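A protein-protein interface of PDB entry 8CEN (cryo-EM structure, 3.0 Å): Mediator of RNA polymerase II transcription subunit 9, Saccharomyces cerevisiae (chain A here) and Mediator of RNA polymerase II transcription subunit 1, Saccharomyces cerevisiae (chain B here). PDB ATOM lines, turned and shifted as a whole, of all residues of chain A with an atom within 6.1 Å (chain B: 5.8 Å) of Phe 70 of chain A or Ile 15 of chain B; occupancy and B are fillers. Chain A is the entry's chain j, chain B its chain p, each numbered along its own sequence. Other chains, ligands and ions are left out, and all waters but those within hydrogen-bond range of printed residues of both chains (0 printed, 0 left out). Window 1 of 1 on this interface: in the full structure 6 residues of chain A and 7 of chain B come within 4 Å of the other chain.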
ATOM      1  N   PHE A  65     -15.227 -15.007 -13.153  1.00  0.00           N
ATOM      2  CA  PHE A  65     -14.327 -15.892 -12.422  1.00  0.00           C
ATOM      3  C   PHE A  65     -14.690 -17.360 -12.576  1.00  0.00           C
ATOM      4  O   PHE A  65     -13.800 -18.196 -12.754  1.00  0.00           O
ATOM      5  CB  PHE A  65     -14.326 -15.516 -10.932  1.00  0.00           C
ATOM      6  CG  PHE A  65     -13.775 -14.149 -10.651  1.00  0.00           C
ATOM      7  CD1 PHE A  65     -12.413 -13.949 -10.507  1.00  0.00           C
ATOM      8  CD2 PHE A  65     -14.625 -13.061 -10.526  1.00  0.00           C
ATOM      9  CE1 PHE A  65     -11.908 -12.688 -10.246  1.00  0.00           C
ATOM     10  CE2 PHE A  65     -14.126 -11.798 -10.265  1.00  0.00           C
ATOM     11  CZ  PHE A  65     -12.766 -11.613 -10.126  1.00  0.00           C
ATOM     12  N   ILE A  66     -15.977 -17.688 -12.516  1.00  0.00           N
ATOM     13  CA  ILE A  66     -16.478 -19.058 -12.629  1.00  0.00           C
ATOM     14  C   ILE A  66     -16.643 -19.619 -14.047  1.00  0.00           C
ATOM     15  O   ILE A  66     -16.463 -20.838 -14.190  1.00  0.00           O
ATOM     16  CB  ILE A  66     -17.785 -19.223 -11.826  1.00  0.00           C
ATOM     17  CG1 ILE A  66     -18.882 -18.259 -12.281  1.00  0.00           C
ATOM     18  CG2 ILE A  66     -17.517 -19.045 -10.336  1.00  0.00           C
ATOM     19  CD1 ILE A  66     -20.196 -18.433 -11.548  1.00  0.00           C
ATOM     20  N   PRO A  67     -17.038 -18.865 -15.099  1.00  0.00           N
ATOM     21  CA  PRO A  67     -17.325 -19.559 -16.372  1.00  0.00           C
ATOM     22  C   PRO A  67     -16.102 -20.182 -17.012  1.00  0.00           C
ATOM     23  O   PRO A  67     -16.191 -21.299 -17.538  1.00  0.00           O
ATOM     24  CB  PRO A  67     -17.925 -18.453 -17.253  1.00  0.00           C
ATOM     25  CG  PRO A  67     -18.355 -17.412 -16.304  1.00  0.00           C
ATOM     26  CD  PRO A  67     -17.272 -17.420 -15.297  1.00  0.00           C
ATOM     27  N   HIS A  68     -14.957 -19.502 -16.939  1.00  0.00           N
ATOM     28  CA  HIS A  68     -13.720 -20.065 -17.461  1.00  0.00           C
ATOM     29  C   HIS A  68     -13.332 -21.332 -16.709  1.00  0.00           C
ATOM     30  O   HIS A  68     -12.912 -22.320 -17.322  1.00  0.00           O
ATOM     31  CB  HIS A  68     -12.602 -19.026 -17.385  1.00  0.00           C
ATOM     32  CG  HIS A  68     -11.306 -19.486 -17.976  1.00  0.00           C
ATOM     33  ND1 HIS A  68     -11.051 -19.442 -19.329  1.00  0.00           N
ATOM     34  CD2 HIS A  68     -10.191 -19.995 -17.400  1.00  0.00           C
ATOM     35  CE1 HIS A  68      -9.836 -19.906 -19.563  1.00  0.00           C
ATOM     36  NE2 HIS A  68      -9.293 -20.248 -18.407  1.00  0.00           N
ATOM     37  N   ILE A  69     -13.503 -21.340 -15.384  1.00  0.00           N
ATOM     38  CA  ILE A  69     -13.051 -22.499 -14.622  1.00  0.00           C
ATOM     39  C   ILE A  69     -13.997 -23.688 -14.799  1.00  0.00           C
ATOM     40  O   ILE A  69     -13.533 -24.835 -14.884  1.00  0.00           O
ATOM     41  CB  ILE A  69     -12.805 -22.146 -13.137  1.00  0.00           C
ATOM     42  CG1 ILE A  69     -14.096 -21.899 -12.356  1.00  0.00           C
ATOM     43  CG2 ILE A  69     -11.872 -20.943 -13.025  1.00  0.00           C
ATOM     44  CD1 ILE A  69     -13.887 -21.766 -10.862  1.00  0.00           C
ATOM     45  N   PHE A  70     -15.324 -23.476 -14.911  1.00  0.00           N
ATOM     46  CA  PHE A  70     -16.099 -24.694 -15.153  1.00  0.00           C
ATOM     47  C   PHE A  70     -16.069 -25.117 -16.616  1.00  0.00           C
ATOM     48  O   PHE A  70     -16.227 -26.311 -16.889  1.00  0.00           O
ATOM     49  CB  PHE A  70     -17.569 -24.676 -14.669  1.00  0.00           C
ATOM     50  CG  PHE A  70     -18.489 -23.695 -15.351  1.00  0.00           C
ATOM     51  CD1 PHE A  70     -19.164 -24.057 -16.507  1.00  0.00           C
ATOM     52  CD2 PHE A  70     -18.893 -22.546 -14.702  1.00  0.00           C
ATOM     53  CE1 PHE A  70     -20.052 -23.196 -17.110  1.00  0.00           C
ATOM     54  CE2 PHE A  70     -19.812 -21.689 -15.282  1.00  0.00           C
ATOM     55  CZ  PHE A  70     -20.389 -22.013 -16.491  1.00  0.00           C
ATOM     56  N   TYR A  71     -15.824 -24.197 -17.555  1.00  0.00           N
ATOM     57  CA  TYR A  71     -15.560 -24.623 -18.924  1.00  0.00           C
ATOM     58  C   TYR A  71     -14.280 -25.445 -18.995  1.00  0.00           C
ATOM     59  O   TYR A  71     -14.222 -26.459 -19.698  1.00  0.00           O
ATOM     60  CB  TYR A  71     -15.481 -23.410 -19.852  1.00  0.00           C
ATOM     61  CG  TYR A  71     -15.324 -23.776 -21.311  1.00  0.00           C
ATOM     62  CD1 TYR A  71     -16.400 -24.263 -22.044  1.00  0.00           C
ATOM     63  CD2 TYR A  71     -14.099 -23.639 -21.953  1.00  0.00           C
ATOM     64  CE1 TYR A  71     -16.261 -24.603 -23.377  1.00  0.00           C
ATOM     65  CE2 TYR A  71     -13.951 -23.976 -23.287  1.00  0.00           C
ATOM     66  CZ  TYR A  71     -15.034 -24.457 -23.993  1.00  0.00           C
ATOM     67  OH  TYR A  71     -14.889 -24.793 -25.320  1.00  0.00           O
ATOM     68  N   SER A  72     -13.255 -25.047 -18.234  1.00  0.00           N
ATOM     69  CA  SER A  72     -12.011 -25.809 -18.203  1.00  0.00           C
ATOM     70  C   SER A  72     -12.206 -27.185 -17.574  1.00  0.00           C
ATOM     71  O   SER A  72     -11.743 -28.194 -18.122  1.00  0.00           O
ATOM     72  CB  SER A  72     -10.942 -25.022 -17.446  1.00  0.00           C
ATOM     73  OG  SER A  72     -10.720 -23.760 -18.049  1.00  0.00           O
ATOM     74  N   LEU A  73     -12.905 -27.256 -16.436  1.00  0.00           N
ATOM     75  CA  LEU A  73     -13.120 -28.556 -15.808  1.00  0.00           C
ATOM     76  C   LEU A  73     -14.134 -29.410 -16.563  1.00  0.00           C
ATOM     77  O   LEU A  73     -14.223 -30.616 -16.302  1.00  0.00           O
ATOM     78  CB  LEU A  73     -13.515 -28.391 -14.335  1.00  0.00           C
ATOM     79  CG  LEU A  73     -14.853 -27.826 -13.860  1.00  0.00           C
ATOM     80  CD1 LEU A  73     -15.890 -28.904 -13.618  1.00  0.00           C
ATOM     81  CD2 LEU A  73     -14.641 -27.010 -12.590  1.00  0.00           C
ATOM     82  N   HIS A  74     -14.909 -28.817 -17.475  1.00  0.00           N
ATOM     83  CA  HIS A  74     -15.636 -29.620 -18.451  1.00  0.00           C
ATOM     84  C   HIS A  74     -14.710 -30.117 -19.558  1.00  0.00           C
ATOM     85  O   HIS A  74     -14.900 -31.225 -20.071  1.00  0.00           O
ATOM     86  CB  HIS A  74     -16.793 -28.811 -19.035  1.00  0.00           C
ATOM     87  CG  HIS A  74     -17.624 -29.567 -20.024  1.00  0.00           C
ATOM     88  ND1 HIS A  74     -17.378 -29.536 -21.380  1.00  0.00           N
ATOM     89  CD2 HIS A  74     -18.700 -30.372 -19.855  1.00  0.00           C
ATOM     90  CE1 HIS A  74     -18.265 -30.290 -22.004  1.00  0.00           C
ATOM     91  NE2 HIS A  74     -19.079 -30.808 -21.101  1.00  0.00           N
ATOM     92  N   GLN A  75     -13.709 -29.313 -19.938  1.00  0.00           N
ATOM     93  CA  GLN A  75     -12.731 -29.739 -20.937  1.00  0.00           C
ATOM     94  C   GLN A  75     -11.808 -30.841 -20.429  1.00  0.00           C
ATOM     95  O   GLN A  75     -11.199 -31.542 -21.245  1.00  0.00           O
ATOM     96  CB  GLN A  75     -11.879 -28.554 -21.405  1.00  0.00           C
ATOM     97  CG  GLN A  75     -12.607 -27.498 -22.231  1.00  0.00           C
ATOM     98  CD  GLN A  75     -13.685 -28.073 -23.125  1.00  0.00           C
ATOM     99  OE1 GLN A  75     -13.391 -28.739 -24.117  1.00  0.00           O
ATOM    100  NE2 GLN A  75     -14.943 -27.821 -22.779  1.00  0.00           N
ATOM    101  N   LEU A  87      -5.836 -27.196 -15.116  1.00  0.00           N
ATOM    102  CA  LEU A  87      -6.689 -26.015 -15.100  1.00  0.00           C
ATOM    103  C   LEU A  87      -5.939 -24.795 -14.574  1.00  0.00           C
ATOM    104  O   LEU A  87      -6.353 -23.662 -14.846  1.00  0.00           O
ATOM    105  CB  LEU A  87      -7.949 -26.309 -14.274  1.00  0.00           C
ATOM    106  CG  LEU A  87      -9.172 -25.382 -14.229  1.00  0.00           C
ATOM    107  CD1 LEU A  87     -10.408 -26.222 -13.949  1.00  0.00           C
ATOM    108  CD2 LEU A  87      -9.080 -24.273 -13.198  1.00  0.00           C
ATOM    109  N   THR B  10     -18.243 -34.941  -7.746  1.00  0.00           N
ATOM    110  CA  THR B  10     -18.079 -33.705  -6.989  1.00  0.00           C
ATOM    111  C   THR B  10     -17.895 -32.487  -7.893  1.00  0.00           C
ATOM    112  O   THR B  10     -18.308 -31.386  -7.510  1.00  0.00           O
ATOM    113  CB  THR B  10     -16.926 -33.815  -5.982  1.00  0.00           C
ATOM    114  OG1 THR B  10     -16.804 -32.580  -5.266  1.00  0.00           O
ATOM    115  CG2 THR B  10     -15.609 -34.123  -6.661  1.00  0.00           C
ATOM    116  N   LEU B  11     -17.325 -32.647  -9.097  1.00  0.00           N
ATOM    117  CA  LEU B  11     -17.302 -31.503 -10.006  1.00  0.00           C
ATOM    118  C   LEU B  11     -18.696 -31.178 -10.527  1.00  0.00           C
ATOM    119  O   LEU B  11     -19.043 -29.995 -10.662  1.00  0.00           O
ATOM    120  CB  LEU B  11     -16.315 -31.723 -11.160  1.00  0.00           C
ATOM    121  CG  LEU B  11     -16.450 -32.781 -12.260  1.00  0.00           C
ATOM    122  CD1 LEU B  11     -17.233 -32.297 -13.480  1.00  0.00           C
ATOM    123  CD2 LEU B  11     -15.058 -33.265 -12.670  1.00  0.00           C
ATOM    124  N   ASP B  12     -19.531 -32.194 -10.756  1.00  0.00           N
ATOM    125  CA  ASP B  12     -20.905 -31.912 -11.137  1.00  0.00           C
ATOM    126  C   ASP B  12     -21.704 -31.325  -9.982  1.00  0.00           C
ATOM    127  O   ASP B  12     -22.546 -30.451 -10.211  1.00  0.00           O
ATOM    128  CB  ASP B  12     -21.572 -33.179 -11.676  1.00  0.00           C
ATOM    129  CG  ASP B  12     -21.060 -33.563 -13.058  1.00  0.00           C
ATOM    130  OD1 ASP B  12     -20.621 -32.662 -13.806  1.00  0.00           O
ATOM    131  OD2 ASP B  12     -21.076 -34.766 -13.389  1.00  0.00           O
ATOM    132  N   SER B  13     -21.385 -31.703  -8.742  1.00  0.00           N
ATOM    133  CA  SER B  13     -22.054 -31.099  -7.596  1.00  0.00           C
ATOM    134  C   SER B  13     -21.637 -29.650  -7.388  1.00  0.00           C
ATOM    135  O   SER B  13     -22.485 -28.817  -7.053  1.00  0.00           O
ATOM    136  CB  SER B  13     -21.767 -31.902  -6.328  1.00  0.00           C
ATOM    137  OG  SER B  13     -20.437 -31.683  -5.893  1.00  0.00           O
ATOM    138  N   MET B  14     -20.359 -29.312  -7.591  1.00  0.00           N
ATOM    139  CA  MET B  14     -19.970 -27.918  -7.384  1.00  0.00           C
ATOM    140  C   MET B  14     -20.449 -27.027  -8.528  1.00  0.00           C
ATOM    141  O   MET B  14     -20.790 -25.861  -8.298  1.00  0.00           O
ATOM    142  CB  MET B  14     -18.460 -27.767  -7.169  1.00  0.00           C
ATOM    143  CG  MET B  14     -17.545 -27.976  -8.361  1.00  0.00           C
ATOM    144  SD  MET B  14     -15.842 -28.086  -7.770  1.00  0.00           S
ATOM    145  CE  MET B  14     -15.008 -28.851  -9.154  1.00  0.00           C
ATOM    146  N   ILE B  15     -20.510 -27.547  -9.763  1.00  0.00           N
ATOM    147  CA  ILE B  15     -21.094 -26.708 -10.808  1.00  0.00           C
ATOM    148  C   ILE B  15     -22.605 -26.592 -10.613  1.00  0.00           C
ATOM    149  O   ILE B  15     -23.195 -25.552 -10.930  1.00  0.00           O
ATOM    150  CB  ILE B  15     -20.729 -27.200 -12.224  1.00  0.00           C
ATOM    151  CG1 ILE B  15     -21.311 -28.581 -12.517  1.00  0.00           C
ATOM    152  CG2 ILE B  15     -19.215 -27.203 -12.401  1.00  0.00           C
ATOM    153  CD1 ILE B  15     -21.195 -29.013 -13.962  1.00  0.00           C
ATOM    154  N   GLU B  16     -23.247 -27.622 -10.044  1.00  0.00           N
ATOM    155  CA  GLU B  16     -24.657 -27.517  -9.676  1.00  0.00           C
ATOM    156  C   GLU B  16     -24.869 -26.476  -8.582  1.00  0.00           C
ATOM    157  O   GLU B  16     -25.852 -25.730  -8.607  1.00  0.00           O
ATOM    158  CB  GLU B  16     -25.176 -28.886  -9.232  1.00  0.00           C
ATOM    159  CG  GLU B  16     -26.590 -28.897  -8.656  1.00  0.00           C
ATOM    160  CD  GLU B  16     -27.658 -28.542  -9.672  1.00  0.00           C
ATOM    161  OE1 GLU B  16     -27.459 -28.810 -10.876  1.00  0.00           O
ATOM    162  OE2 GLU B  16     -28.707 -28.003  -9.262  1.00  0.00           O
ATOM    163  N   LEU B  17     -23.951 -26.411  -7.618  1.00  0.00           N
ATOM    164  CA  LEU B  17     -24.064 -25.440  -6.535  1.00  0.00           C
ATOM    165  C   LEU B  17     -23.835 -24.015  -7.037  1.00  0.00           C
ATOM    166  O   LEU B  17     -24.521 -23.075  -6.602  1.00  0.00           O
ATOM    167  CB  LEU B  17     -23.074 -25.808  -5.430  1.00  0.00           C
ATOM    168  CG  LEU B  17     -23.040 -24.986  -4.147  1.00  0.00           C
ATOM    169  CD1 LEU B  17     -24.366 -25.083  -3.406  1.00  0.00           C
ATOM    170  CD2 LEU B  17     -21.888 -25.432  -3.258  1.00  0.00           C
ATOM    171  N   PHE B  18     -22.874 -23.836  -7.953  1.00  0.00           N
ATOM    172  CA  PHE B  18     -22.676 -22.537  -8.596  1.00  0.00           C
ATOM    173  C   PHE B  18     -23.896 -22.140  -9.420  1.00  0.00           C
ATOM    174  O   PHE B  18     -24.259 -20.959  -9.480  1.00  0.00           O
ATOM    175  CB  PHE B  18     -21.424 -22.548  -9.485  1.00  0.00           C
ATOM    176  CG  PHE B  18     -20.111 -22.736  -8.745  1.00  0.00           C
ATOM    177  CD1 PHE B  18     -20.044 -22.774  -7.356  1.00  0.00           C
ATOM    178  CD2 PHE B  18     -18.933 -22.883  -9.464  1.00  0.00           C
ATOM    179  CE1 PHE B  18     -18.836 -22.952  -6.707  1.00  0.00           C
ATOM    180  CE2 PHE B  18     -17.721 -23.061  -8.818  1.00  0.00           C
ATOM    181  CZ  PHE B  18     -17.674 -23.095  -7.439  1.00  0.00           C
ATOM    182  N   LYS B  19     -24.526 -23.116 -10.080  1.00  0.00           N
ATOM    183  CA  LYS B  19     -25.787 -22.877 -10.774  1.00  0.00           C
ATOM    184  C   LYS B  19     -26.885 -22.449  -9.806  1.00  0.00           C
ATOM    185  O   LYS B  19     -27.670 -21.540 -10.104  1.00  0.00           O
ATOM    186  CB  LYS B  19     -26.209 -24.149 -11.508  1.00  0.00           C
ATOM    187  CG  LYS B  19     -27.431 -23.992 -12.372  1.00  0.00           C
ATOM    188  CD  LYS B  19     -27.801 -25.295 -13.055  1.00  0.00           C
ATOM    189  CE  LYS B  19     -26.821 -25.647 -14.136  1.00  0.00           C
ATOM    190  NZ  LYS B  19     -26.930 -24.656 -15.239  1.00  0.00           N
ATOM    191  N   ASP B  20     -26.956 -23.103  -8.646  1.00  0.00           N
ATOM    192  CA  ASP B  20     -28.034 -22.852  -7.696  1.00  0.00           C
ATOM    193  C   ASP B  20     -27.889 -21.504  -7.003  1.00  0.00           C
ATOM    194  O   ASP B  20     -28.899 -20.889  -6.643  1.00  0.00           O
ATOM    195  CB  ASP B  20     -28.085 -23.972  -6.655  1.00  0.00           C
ATOM    196  CG  ASP B  20     -29.463 -24.136  -6.042  1.00  0.00           C
ATOM    197  OD1 ASP B  20     -30.390 -23.406  -6.451  1.00  0.00           O
ATOM    198  OD2 ASP B  20     -29.617 -24.990  -5.143  1.00  0.00           O
ATOM    199  N   ARG B  33     -24.236 -19.642 -21.518  1.00  0.00           N
ATOM    200  CA  ARG B  33     -23.460 -20.506 -20.631  1.00  0.00           C
ATOM    201  C   ARG B  33     -24.355 -21.236 -19.633  1.00  0.00           C
ATOM    202  O   ARG B  33     -24.078 -22.395 -19.300  1.00  0.00           O
ATOM    203  CB  ARG B  33     -22.360 -19.727 -19.899  1.00  0.00           C
ATOM    204  CG  ARG B  33     -22.783 -18.608 -18.958  1.00  0.00           C
ATOM    205  CD  ARG B  33     -21.586 -17.702 -18.680  1.00  0.00           C
ATOM    206  NE  ARG B  33     -21.928 -16.495 -17.938  1.00  0.00           N
ATOM    207  CZ  ARG B  33     -21.117 -15.457 -17.782  1.00  0.00           C
ATOM    208  NH1 ARG B  33     -19.940 -15.403 -18.383  1.00  0.00           N
ATOM    209  NH2 ARG B  33     -21.509 -14.434 -17.027  1.00  0.00           N
ATOM    210  N   THR B  37     -24.198 -25.346 -19.474  1.00  0.00           N
ATOM    211  CA  THR B  37     -23.707 -26.094 -18.312  1.00  0.00           C
ATOM    212  C   THR B  37     -24.179 -27.545 -18.320  1.00  0.00           C
ATOM    213  O   THR B  37     -23.388 -28.466 -18.082  1.00  0.00           O
ATOM    214  CB  THR B  37     -24.157 -25.425 -17.013  1.00  0.00           C
ATOM    215  OG1 THR B  37     -25.572 -25.212 -17.058  1.00  0.00           O
ATOM    216  CG2 THR B  37     -23.425 -24.130 -16.744  1.00  0.00           C
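Pro 67 of chain A touches Arg 33 of chain B (CG to NH1, 3.3 Å). Phe 70 of chain A touches Ile 15 of chain B (CB to CG2, 3.8 Å). Thr 37 of chain B touches Phe 70 of chain A. Leu 73 of chain A touches Leu 11 of chain B (CD1 to CD1, 3.7 Å). Leu 73 of chain A touches Met 14 of chain B. Ile 15 of chain B touches Leu 73 of chain A (CG2 to CD1, 3.9 Å).
Phe 70 of chain A touches two residues of chain B. Printed residues of chain B within 4 Å of Leu 73 of chain A: Leu 11, Met 14 and Ile 15. Of chain A, only Phe 70 and Leu 73 come within 4 Å of Ile 15 of chain B. Glu 16 of chain B touches none of the printed residues of chain A. Printed residues of chain A within 4 Å of Thr 37 of chain B: Phe 70 (3.5 Å). The nearest residue of chain B that does not touch Phe 70 of chain A is Arg 33 of chain B (4.6 Å). The nearest printed residue of chain A that does not touch Arg 33 of chain B is Phe 70 of chain A (4.6 Å).
Printed residues of chain B that touch a printed residue of chain A: Leu 11, Met 14, Ile 15, Arg 33 and Thr 37. Of the 12 printed residues of chain A, 3 touch a printed residue of chain B. Hydrophobic or aromatic side chains of chain A that line the printed part of chain B: Pro 67, Phe 70 and Leu 73.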
